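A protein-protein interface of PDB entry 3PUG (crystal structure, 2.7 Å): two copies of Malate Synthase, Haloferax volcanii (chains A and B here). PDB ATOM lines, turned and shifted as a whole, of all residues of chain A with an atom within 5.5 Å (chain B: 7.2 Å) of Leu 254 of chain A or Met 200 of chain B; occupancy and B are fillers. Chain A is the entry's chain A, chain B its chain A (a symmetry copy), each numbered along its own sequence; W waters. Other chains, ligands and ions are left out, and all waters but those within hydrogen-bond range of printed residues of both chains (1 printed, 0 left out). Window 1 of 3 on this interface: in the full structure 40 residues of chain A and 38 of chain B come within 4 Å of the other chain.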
ATOM      1  N   PHE A  10      27.060 -26.564  -6.365  1.00  0.00           N
ATOM      2  CA  PHE A  10      25.967 -25.898  -7.095  1.00  0.00           C
ATOM      3  C   PHE A  10      24.663 -25.886  -6.294  1.00  0.00           C
ATOM      4  O   PHE A  10      24.469 -26.746  -5.438  1.00  0.00           O
ATOM      5  CB  PHE A  10      25.591 -26.657  -8.362  1.00  0.00           C
ATOM      6  CG  PHE A  10      26.677 -26.759  -9.384  1.00  0.00           C
ATOM      7  CD1 PHE A  10      26.740 -25.852 -10.438  1.00  0.00           C
ATOM      8  CD2 PHE A  10      27.633 -27.771  -9.322  1.00  0.00           C
ATOM      9  CE1 PHE A  10      27.725 -25.964 -11.432  1.00  0.00           C
ATOM     10  CE2 PHE A  10      28.617 -27.874 -10.297  1.00  0.00           C
ATOM     11  CZ  PHE A  10      28.661 -26.979 -11.369  1.00  0.00           C
ATOM     12  N   VAL A  11      23.716 -25.007  -6.611  1.00  0.00           N
ATOM     13  CA  VAL A  11      22.488 -24.892  -5.849  1.00  0.00           C
ATOM     14  C   VAL A  11      21.532 -24.434  -6.919  1.00  0.00           C
ATOM     15  O   VAL A  11      21.779 -23.383  -7.464  1.00  0.00           O
ATOM     16  CB  VAL A  11      22.574 -23.768  -4.807  1.00  0.00           C
ATOM     17  CG1 VAL A  11      21.208 -23.188  -4.468  1.00  0.00           C
ATOM     18  CG2 VAL A  11      23.275 -24.238  -3.574  1.00  0.00           C
ATOM     19  N   ARG A  12      20.482 -25.196  -7.239  1.00  0.00           N
ATOM     20  CA  ARG A  12      19.565 -24.936  -8.342  1.00  0.00           C
ATOM     21  C   ARG A  12      18.352 -24.192  -7.837  1.00  0.00           C
ATOM     22  O   ARG A  12      17.826 -23.308  -8.518  1.00  0.00           O
ATOM     23  CB  ARG A  12      19.064 -26.247  -8.949  1.00  0.00           C
ATOM     24  CG  ARG A  12      20.165 -27.152  -9.499  1.00  0.00           C
ATOM     25  CD  ARG A  12      19.755 -28.609  -9.659  1.00  0.00           C
ATOM     26  NE  ARG A  12      19.599 -29.216  -8.359  1.00  0.00           N
ATOM     27  CZ  ARG A  12      18.858 -30.300  -8.142  1.00  0.00           C
ATOM     28  NH1 ARG A  12      18.248 -30.892  -9.160  1.00  0.00           N
ATOM     29  NH2 ARG A  12      18.731 -30.803  -6.927  1.00  0.00           N
ATOM     30  N   ALA A 227      26.302 -18.116  -7.420  1.00  0.00           N
ATOM     31  CA  ALA A 227      25.288 -17.109  -7.772  1.00  0.00           C
ATOM     32  C   ALA A 227      23.887 -17.702  -7.935  1.00  0.00           C
ATOM     33  O   ALA A 227      23.740 -18.768  -8.534  1.00  0.00           O
ATOM     34  CB  ALA A 227      25.693 -16.368  -9.066  1.00  0.00           C
ATOM     35  N   THR A 246      17.001 -20.416 -18.239  1.00  0.00           N
ATOM     36  CA  THR A 246      17.844 -20.586 -19.389  1.00  0.00           C
ATOM     37  C   THR A 246      18.688 -19.307 -19.626  1.00  0.00           C
ATOM     38  O   THR A 246      19.904 -19.422 -19.861  1.00  0.00           O
ATOM     39  CB  THR A 246      16.979 -21.034 -20.611  1.00  0.00           C
ATOM     40  OG1 THR A 246      16.663 -22.432 -20.472  1.00  0.00           O
ATOM     41  CG2 THR A 246      17.686 -20.781 -21.935  1.00  0.00           C
ATOM     42  N   ASN A 248      19.668 -17.013 -17.409  1.00  0.00           N
ATOM     43  CA  ASN A 248      20.580 -17.003 -16.283  1.00  0.00           C
ATOM     44  C   ASN A 248      21.686 -18.016 -16.515  1.00  0.00           C
ATOM     45  O   ASN A 248      22.850 -17.810 -16.133  1.00  0.00           O
ATOM     46  CB  ASN A 248      19.903 -17.401 -14.960  1.00  0.00           C
ATOM     47  CG  ASN A 248      18.892 -16.369 -14.463  1.00  0.00           C
ATOM     48  OD1 ASN A 248      18.876 -15.201 -14.874  1.00  0.00           O
ATOM     49  ND2 ASN A 248      18.009 -16.817 -13.569  1.00  0.00           N
ATOM     50  N   GLN A 249      21.324 -19.161 -17.080  1.00  0.00           N
ATOM     51  CA  GLN A 249      22.305 -20.236 -17.191  1.00  0.00           C
ATOM     52  C   GLN A 249      23.328 -19.768 -18.209  1.00  0.00           C
ATOM     53  O   GLN A 249      24.475 -20.192 -18.186  1.00  0.00           O
ATOM     54  CB  GLN A 249      21.639 -21.555 -17.556  1.00  0.00           C
ATOM     55  CG  GLN A 249      20.828 -22.163 -16.380  1.00  0.00           C
ATOM     56  CD  GLN A 249      19.641 -23.032 -16.815  1.00  0.00           C
ATOM     57  OE1 GLN A 249      19.551 -23.452 -17.983  1.00  0.00           O
ATOM     58  NE2 GLN A 249      18.684 -23.244 -15.894  1.00  0.00           N
ATOM     59  N   ALA A 250      22.981 -18.800 -19.046  1.00  0.00           N
ATOM     60  CA  ALA A 250      23.941 -18.399 -20.058  1.00  0.00           C
ATOM     61  C   ALA A 250      24.858 -17.315 -19.489  1.00  0.00           C
ATOM     62  O   ALA A 250      25.795 -16.850 -20.151  1.00  0.00           O
ATOM     63  CB  ALA A 250      23.216 -17.913 -21.280  1.00  0.00           C
ATOM     64  N   GLY A 252      26.050 -17.917 -16.352  1.00  0.00           N
ATOM     65  CA  GLY A 252      26.665 -18.691 -15.278  1.00  0.00           C
ATOM     66  C   GLY A 252      25.903 -18.499 -13.958  1.00  0.00           C
ATOM     67  O   GLY A 252      26.431 -18.830 -12.881  1.00  0.00           O
ATOM     68  N   MET A 253      24.687 -17.953 -14.001  1.00  0.00           N
ATOM     69  CA  MET A 253      23.839 -18.007 -12.842  1.00  0.00           C
ATOM     70  C   MET A 253      22.897 -19.227 -12.885  1.00  0.00           C
ATOM     71  O   MET A 253      21.879 -19.258 -13.609  1.00  0.00           O
ATOM     72  CB  MET A 253      23.056 -16.708 -12.787  1.00  0.00           C
ATOM     73  CG  MET A 253      22.194 -16.534 -11.553  1.00  0.00           C
ATOM     74  SD  MET A 253      21.550 -14.854 -11.584  1.00  0.00           S
ATOM     75  CE  MET A 253      22.866 -14.258 -10.481  1.00  0.00           C
ATOM     76  N   LEU A 254      23.230 -20.224 -12.079  1.00  0.00           N
ATOM     77  CA  LEU A 254      22.656 -21.546 -12.227  1.00  0.00           C
ATOM     78  C   LEU A 254      21.515 -21.975 -11.280  1.00  0.00           C
ATOM     79  O   LEU A 254      20.959 -23.049 -11.486  1.00  0.00           O
ATOM     80  CB  LEU A 254      23.793 -22.571 -12.135  1.00  0.00           C
ATOM     81  CG  LEU A 254      24.780 -22.487 -13.293  1.00  0.00           C
ATOM     82  CD1 LEU A 254      25.697 -23.709 -13.192  1.00  0.00           C
ATOM     83  CD2 LEU A 254      24.137 -22.462 -14.663  1.00  0.00           C
ATOM     84  N   GLY A 255      21.254 -21.234 -10.205  1.00  0.00           N
ATOM     85  CA  GLY A 255      20.152 -21.481  -9.281  1.00  0.00           C
ATOM     86  C   GLY A 255      19.229 -20.280  -9.388  1.00  0.00           C
ATOM     87  O   GLY A 255      19.543 -19.217  -9.947  1.00  0.00           O
ATOM     88  N   ILE A 256      18.038 -20.428  -8.851  1.00  0.00           N
ATOM     89  CA  ILE A 256      17.129 -19.313  -8.884  1.00  0.00           C
ATOM     90  C   ILE A 256      16.168 -19.507  -7.713  1.00  0.00           C
ATOM     91  O   ILE A 256      16.051 -20.612  -7.152  1.00  0.00           O
ATOM     92  CB  ILE A 256      16.388 -19.313 -10.212  1.00  0.00           C
ATOM     93  CG1 ILE A 256      15.382 -18.167 -10.276  1.00  0.00           C
ATOM     94  CG2 ILE A 256      15.704 -20.702 -10.437  1.00  0.00           C
ATOM     95  CD1 ILE A 256      15.008 -17.875 -11.683  1.00  0.00           C
ATOM     96  N   SER A 270      15.300 -27.757 -14.808  1.00  0.00           N
ATOM     97  CA  SER A 270      15.871 -26.897 -15.839  1.00  0.00           C
ATOM     98  C   SER A 270      17.392 -26.938 -16.064  1.00  0.00           C
ATOM     99  O   SER A 270      17.802 -27.103 -17.203  1.00  0.00           O
ATOM    100  CB  SER A 270      15.412 -25.446 -15.727  1.00  0.00           C
ATOM    101  OG  SER A 270      16.299 -24.741 -16.564  1.00  0.00           O
ATOM    102  N   PRO A 271      18.230 -26.750 -15.030  1.00  0.00           N
ATOM    103  CA  PRO A 271      19.669 -26.810 -15.353  1.00  0.00           C
ATOM    104  C   PRO A 271      20.248 -28.200 -15.693  1.00  0.00           C
ATOM    105  O   PRO A 271      21.387 -28.295 -16.186  1.00  0.00           O
ATOM    106  CB  PRO A 271      20.348 -26.202 -14.115  1.00  0.00           C
ATOM    107  CG  PRO A 271      19.409 -26.498 -13.022  1.00  0.00           C
ATOM    108  CD  PRO A 271      18.001 -26.508 -13.600  1.00  0.00           C
ATOM    109  N   LEU A 272      19.485 -29.264 -15.438  1.00  0.00           N
ATOM    110  CA  LEU A 272      19.842 -30.628 -15.875  1.00  0.00           C
ATOM    111  C   LEU A 272      19.719 -30.818 -17.391  1.00  0.00           C
ATOM    112  O   LEU A 272      18.862 -30.197 -18.036  1.00  0.00           O
ATOM    113  CB  LEU A 272      18.957 -31.629 -15.153  1.00  0.00           C
ATOM    114  CG  LEU A 272      19.155 -31.608 -13.636  1.00  0.00           C
ATOM    115  CD1 LEU A 272      18.183 -32.560 -12.953  1.00  0.00           C
ATOM    116  CD2 LEU A 272      20.592 -31.925 -13.242  1.00  0.00           C
ATOM    117  N   THR B 194      33.760 -18.662 -20.435  1.00  0.00           N
ATOM    118  CA  THR B 194      32.514 -19.411 -20.238  1.00  0.00           C
ATOM    119  C   THR B 194      32.657 -20.527 -19.230  1.00  0.00           C
ATOM    120  O   THR B 194      31.901 -20.569 -18.245  1.00  0.00           O
ATOM    121  CB  THR B 194      31.917 -19.929 -21.525  1.00  0.00           C
ATOM    122  OG1 THR B 194      31.682 -18.787 -22.362  1.00  0.00           O
ATOM    123  CG2 THR B 194      30.573 -20.673 -21.271  1.00  0.00           C
ATOM    124  N   MET B 197      33.082 -18.845 -15.568  1.00  0.00           N
ATOM    125  CA  MET B 197      31.808 -18.333 -15.102  1.00  0.00           C
ATOM    126  C   MET B 197      30.779 -19.455 -14.943  1.00  0.00           C
ATOM    127  O   MET B 197      29.651 -19.195 -14.504  1.00  0.00           O
ATOM    128  CB  MET B 197      31.247 -17.263 -16.033  1.00  0.00           C
ATOM    129  CG  MET B 197      32.081 -16.000 -16.221  1.00  0.00           C
ATOM    130  SD  MET B 197      31.862 -14.878 -14.802  1.00  0.00           S
ATOM    131  CE  MET B 197      30.259 -14.132 -15.238  1.00  0.00           C
ATOM    132  N   ARG B 198      31.150 -20.708 -15.214  1.00  0.00           N
ATOM    133  CA  ARG B 198      30.208 -21.854 -15.198  1.00  0.00           C
ATOM    134  C   ARG B 198      28.904 -21.593 -15.940  1.00  0.00           C
ATOM    135  O   ARG B 198      27.846 -21.939 -15.475  1.00  0.00           O
ATOM    136  CB  ARG B 198      29.920 -22.351 -13.788  1.00  0.00           C
ATOM    137  CG  ARG B 198      31.137 -22.456 -12.837  1.00  0.00           C
ATOM    138  CD  ARG B 198      30.852 -23.355 -11.641  1.00  0.00           C
ATOM    139  NE  ARG B 198      29.795 -22.848 -10.752  1.00  0.00           N
ATOM    140  CZ  ARG B 198      29.429 -23.433  -9.609  1.00  0.00           C
ATOM    141  NH1 ARG B 198      30.046 -24.544  -9.187  1.00  0.00           N
ATOM    142  NH2 ARG B 198      28.474 -22.885  -8.864  1.00  0.00           N
ATOM    143  N   ALA B 199      28.971 -20.970 -17.102  1.00  0.00           N
ATOM    144  CA  ALA B 199      27.784 -20.706 -17.880  1.00  0.00           C
ATOM    145  C   ALA B 199      27.520 -21.939 -18.753  1.00  0.00           C
ATOM    146  O   ALA B 199      28.440 -22.746 -19.002  1.00  0.00           O
ATOM    147  CB  ALA B 199      28.008 -19.456 -18.737  1.00  0.00           C
ATOM    148  N   MET B 200      26.271 -22.104 -19.189  1.00  0.00           N
ATOM    149  CA  MET B 200      25.940 -23.178 -20.101  1.00  0.00           C
ATOM    150  C   MET B 200      24.842 -22.773 -21.067  1.00  0.00           C
ATOM    151  O   MET B 200      23.915 -22.056 -20.702  1.00  0.00           O
ATOM    152  CB  MET B 200      25.647 -24.466 -19.338  1.00  0.00           C
ATOM    153  CG  MET B 200      24.286 -24.592 -18.690  1.00  0.00           C
ATOM    154  SD  MET B 200      24.198 -25.966 -17.474  1.00  0.00           S
ATOM    155  CE  MET B 200      22.730 -25.282 -16.681  1.00  0.00           C
ATOM    156  N   THR B 201      24.959 -23.191 -22.321  1.00  0.00           N
ATOM    157  CA  THR B 201      23.882 -22.936 -23.286  1.00  0.00           C
ATOM    158  C   THR B 201      23.289 -24.260 -23.786  1.00  0.00           C
ATOM    159  O   THR B 201      24.009 -25.251 -23.840  1.00  0.00           O
ATOM    160  CB  THR B 201      24.400 -22.124 -24.481  1.00  0.00           C
ATOM    161  OG1 THR B 201      25.603 -22.735 -24.944  1.00  0.00           O
ATOM    162  CG2 THR B 201      24.660 -20.717 -24.090  1.00  0.00           C
ATOM    163  N   PRO B 202      21.999 -24.282 -24.175  1.00  0.00           N
ATOM    164  CA  PRO B 202      21.393 -25.537 -24.633  1.00  0.00           C
ATOM    165  C   PRO B 202      22.091 -26.108 -25.869  1.00  0.00           C
ATOM    166  O   PRO B 202      22.358 -27.299 -25.894  1.00  0.00           O
ATOM    167  CB  PRO B 202      19.962 -25.122 -24.970  1.00  0.00           C
ATOM    168  CG  PRO B 202      19.730 -23.819 -24.242  1.00  0.00           C
ATOM    169  CD  PRO B 202      21.067 -23.159 -24.399  1.00  0.00           C
ATOM    170  N   THR B 203      22.475 -25.297 -26.850  1.00  0.00           N
ATOM    171  CA  THR B 203      23.296 -25.826 -27.943  1.00  0.00           C
ATOM    172  C   THR B 203      24.759 -26.038 -27.590  1.00  0.00           C
ATOM    173  O   THR B 203      25.430 -26.752 -28.330  1.00  0.00           O
ATOM    174  CB  THR B 203      23.250 -24.989 -29.246  1.00  0.00           C
ATOM    175  OG1 THR B 203      24.044 -23.804 -29.118  1.00  0.00           O
ATOM    176  CG2 THR B 203      21.813 -24.573 -29.620  1.00  0.00           C
ATOM    177  N   GLY B 204      25.282 -25.431 -26.512  1.00  0.00           N
ATOM    178  CA  GLY B 204      26.751 -25.383 -26.269  1.00  0.00           C
ATOM    179  C   GLY B 204      27.506 -24.349 -27.119  1.00  0.00           C
ATOM    180  O   GLY B 204      28.730 -24.324 -27.134  1.00  0.00           O
ATOM    181  N   GLU B 205      26.808 -23.477 -27.851  1.00  0.00           N
ATOM    182  CA  GLU B 205      27.464 -22.346 -28.530  1.00  0.00           C
ATOM    183  C   GLU B 205      27.811 -21.269 -27.477  1.00  0.00           C
ATOM    184  O   GLU B 205      27.102 -21.113 -26.487  1.00  0.00           O
ATOM    185  CB  GLU B 205      26.649 -21.792 -29.725  1.00  0.00           C
ATOM    186  CG  GLU B 205      25.508 -20.820 -29.449  1.00  0.00           C
ATOM    187  CD  GLU B 205      25.243 -19.742 -30.546  1.00  0.00           C
ATOM    188  OE1 GLU B 205      26.161 -18.978 -30.977  1.00  0.00           O
ATOM    189  OE2 GLU B 205      24.059 -19.577 -30.940  1.00  0.00           O
ATOM    190  N   PRO B 207      27.717 -18.285 -25.156  1.00  0.00           N
ATOM    191  CA  PRO B 207      26.931 -17.062 -24.876  1.00  0.00           C
ATOM    192  C   PRO B 207      27.667 -15.813 -25.425  1.00  0.00           C
ATOM    193  O   PRO B 207      28.899 -15.841 -25.617  1.00  0.00           O
ATOM    194  CB  PRO B 207      26.889 -16.996 -23.347  1.00  0.00           C
ATOM    195  CG  PRO B 207      27.556 -18.287 -22.841  1.00  0.00           C
ATOM    196  CD  PRO B 207      28.277 -18.941 -23.966  1.00  0.00           C
ATOM    197  N   TRP B 209      27.965 -12.532 -24.174  1.00  0.00           N
ATOM    198  CA  TRP B 209      28.660 -11.802 -23.092  1.00  0.00           C
ATOM    199  C   TRP B 209      28.855 -10.361 -23.503  1.00  0.00           C
ATOM    200  O   TRP B 209      29.980  -9.846 -23.539  1.00  0.00           O
ATOM    201  CB  TRP B 209      30.026 -12.393 -22.814  1.00  0.00           C
ATOM    202  CG  TRP B 209      30.070 -13.806 -22.336  1.00  0.00           C
ATOM    203  CD1 TRP B 209      30.620 -14.873 -22.984  1.00  0.00           C
ATOM    204  CD2 TRP B 209      29.610 -14.304 -21.065  1.00  0.00           C
ATOM    205  NE1 TRP B 209      30.471 -16.026 -22.224  1.00  0.00           N
ATOM    206  CE2 TRP B 209      29.864 -15.696 -21.041  1.00  0.00           C
ATOM    207  CE3 TRP B 209      28.950 -13.723 -19.978  1.00  0.00           C
ATOM    208  CZ2 TRP B 209      29.547 -16.489 -19.946  1.00  0.00           C
ATOM    209  CZ3 TRP B 209      28.607 -14.520 -18.898  1.00  0.00           C
ATOM    210  CH2 TRP B 209      28.888 -15.899 -18.908  1.00  0.00           C
ATOM    211  N   ALA B 394      33.522 -27.429 -21.456  1.00  0.00           N
ATOM    212  CA  ALA B 394      32.178 -26.873 -21.639  1.00  0.00           C
ATOM    213  C   ALA B 394      31.088 -27.824 -21.160  1.00  0.00           C
ATOM    214  O   ALA B 394      30.316 -27.465 -20.272  1.00  0.00           O
ATOM    215  CB  ALA B 394      31.923 -26.471 -23.080  1.00  0.00           C
ATOM    216  N   THR B 397      30.221 -29.014 -17.383  1.00  0.00           N
ATOM    217  CA  THR B 397      29.496 -28.148 -16.474  1.00  0.00           C
ATOM    218  C   THR B 397      28.153 -28.756 -16.073  1.00  0.00           C
ATOM    219  O   THR B 397      27.913 -28.890 -14.884  1.00  0.00           O
ATOM    220  CB  THR B 397      29.373 -26.703 -17.020  1.00  0.00           C
ATOM    221  OG1 THR B 397      30.668 -26.112 -17.060  1.00  0.00           O
ATOM    222  CG2 THR B 397      28.517 -25.879 -16.118  1.00  0.00           C
ATOM    223  N   PRO B 398      27.272 -29.065 -17.048  1.00  0.00           N
ATOM    224  CA  PRO B 398      26.012 -29.698 -16.740  1.00  0.00           C
ATOM    225  C   PRO B 398      26.310 -31.052 -16.130  1.00  0.00           C
ATOM    226  O   PRO B 398      25.671 -31.408 -15.156  1.00  0.00           O
ATOM    227  CB  PRO B 398      25.366 -29.892 -18.100  1.00  0.00           C
ATOM    228  CG  PRO B 398      26.020 -28.905 -18.989  1.00  0.00           C
ATOM    229  CD  PRO B 398      27.395 -28.759 -18.485  1.00  0.00           C
ATOM    230  N   ILE B 399      27.289 -31.798 -16.636  1.00  0.00           N
ATOM    231  CA  ILE B 399      27.664 -33.052 -15.992  1.00  0.00           C
ATOM    232  C   ILE B 399      28.094 -32.794 -14.559  1.00  0.00           C
ATOM    233  O   ILE B 399      27.582 -33.462 -13.669  1.00  0.00           O
ATOM    234  CB  ILE B 399      28.758 -33.824 -16.764  1.00  0.00           C
ATOM    235  CG1 ILE B 399      28.167 -34.571 -17.953  1.00  0.00           C
ATOM    236  CG2 ILE B 399      29.379 -34.885 -15.899  1.00  0.00           C
ATOM    237  CD1 ILE B 399      27.183 -33.790 -18.754  1.00  0.00           C
ATOM    238  N   LEU B 401      27.249 -30.335 -12.557  1.00  0.00           N
ATOM    239  CA  LEU B 401      26.086 -29.945 -11.808  1.00  0.00           C
ATOM    240  C   LEU B 401      25.300 -31.225 -11.547  1.00  0.00           C
ATOM    241  O   LEU B 401      24.684 -31.403 -10.494  1.00  0.00           O
ATOM    242  CB  LEU B 401      25.242 -28.911 -12.562  1.00  0.00           C
ATOM    243  CG  LEU B 401      23.782 -28.801 -12.086  1.00  0.00           C
ATOM    244  CD1 LEU B 401      23.554 -27.857 -10.961  1.00  0.00           C
ATOM    245  CD2 LEU B 401      22.976 -28.291 -13.213  1.00  0.00           C
HETATM  246  O   HOH W   1      21.590 -20.847 -21.431  1.00  0.00           O
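O of Gln 249 of chain A lies within hydrogen-bond range of N of Met 200 of chain B, at 2.8 Å.
N of Ile 256 of chain A sits at hydrogen-bond distance from O of Arg 12 of chain A (2.9 Å). The side-chain amide nitrogen (NE2) of Gln 249 of chain A sits at hydrogen-bond distance from the side-chain hydroxyl (OG) of Ser 270 of chain A (2.9 Å). O of Thr 194 of chain B sits at hydrogen-bond distance from N of Ala 199 of chain B. The indole nitrogen (NE1) of Trp 209 of chain B sits at hydrogen-bond distance from the side-chain hydroxyl (OG1) of Thr 194 of chain B, at 3.0 Å.
Among the printed residues, merely in contact across the chains: Gly 252 of chain A with Met 197 of chain B, Pro 271 of chain A with Met 200 of chain B, Gln 249 of chain A with Ala 199 of chain B, Pro 271 of chain A with Leu 401 of chain B, Ala 250 of chain A with Pro 207 of chain B, Gly 252 of chain A with Ala 199 of chain B, Gly 252 of chain A with Arg 198 of chain B, Ala 250 of chain A with Trp 209 of chain B, Phe 10 of chain A with Leu 401 of chain B, Phe 10 of chain A with Arg 198 of chain B, Leu 254 of chain A with Arg 198 of chain B, Ala 250 of chain A with Ala 199 of chain B, Ala 250 of chain A with Met 200 of chain B, Leu 254 of chain A with Met 200 of chain B and Arg 12 of chain A with Leu 401 of chain B.
Leu 254 of chain A touches just these residues of chain B: Arg 198 and Met 200. Met 200 of chain B touches just these residues of chain A: Gln 249, Ala 250, Leu 254 and Pro 271. Printed residues of chain A within 4 Å of Arg 198 of chain B: Phe 10 (3.5 Å), Gly 252 (3.5 Å) and Leu 254 (3.6 Å). Printed residues of chain A within 4 Å of Pro 207 of chain B: Ala 250. Printed residues of chain B within 4 Å of Gln 249 of chain A: Ala 199 and Met 200. Printed residues of chain A within 4 Å of Ala 199 of chain B: Gln 249 (3.4 Å), Ala 250 (3.7 Å) and Gly 252 (3.4 Å). The nearest residue of chain B that does not touch Leu 254 of chain A is Thr 397 of chain B (4.6 Å). The nearest printed residue of chain A that does not touch Pro 207 of chain B is Gln 249 of chain A (5.9 Å).
Of the 17 printed residues of chain B, 7 touch a printed residue of chain A. Hydrophobic or aromatic side chains of chain B that line the printed part of chain A: Ala 199, Met 200, Pro 207, Trp 209 and Leu 401. Along chain B the printed residues that touch a printed residue of chain A span positions 197 to 401. Of the 16 printed residues of chain A, 7 touch a printed residue of chain B. Among the printed residues, 16 pairs touch across the chains. Among the printed residues, no Asp or Glu carboxylate lies within 4 Å of a Lys or Arg side-chain nitrogen of the other chain.
No position is printed for both chains. Of the 16 pairs that touch across the chains among the printed residues, none has its exchanged pair printed and touching as well.
Water W1 lies within hydrogen-bond range of O of Thr 246 of chain A (2.7 Å), O of Met 200 of chain B (2.7 Å) and N of Ala 250 of chain A (3.4 Å).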
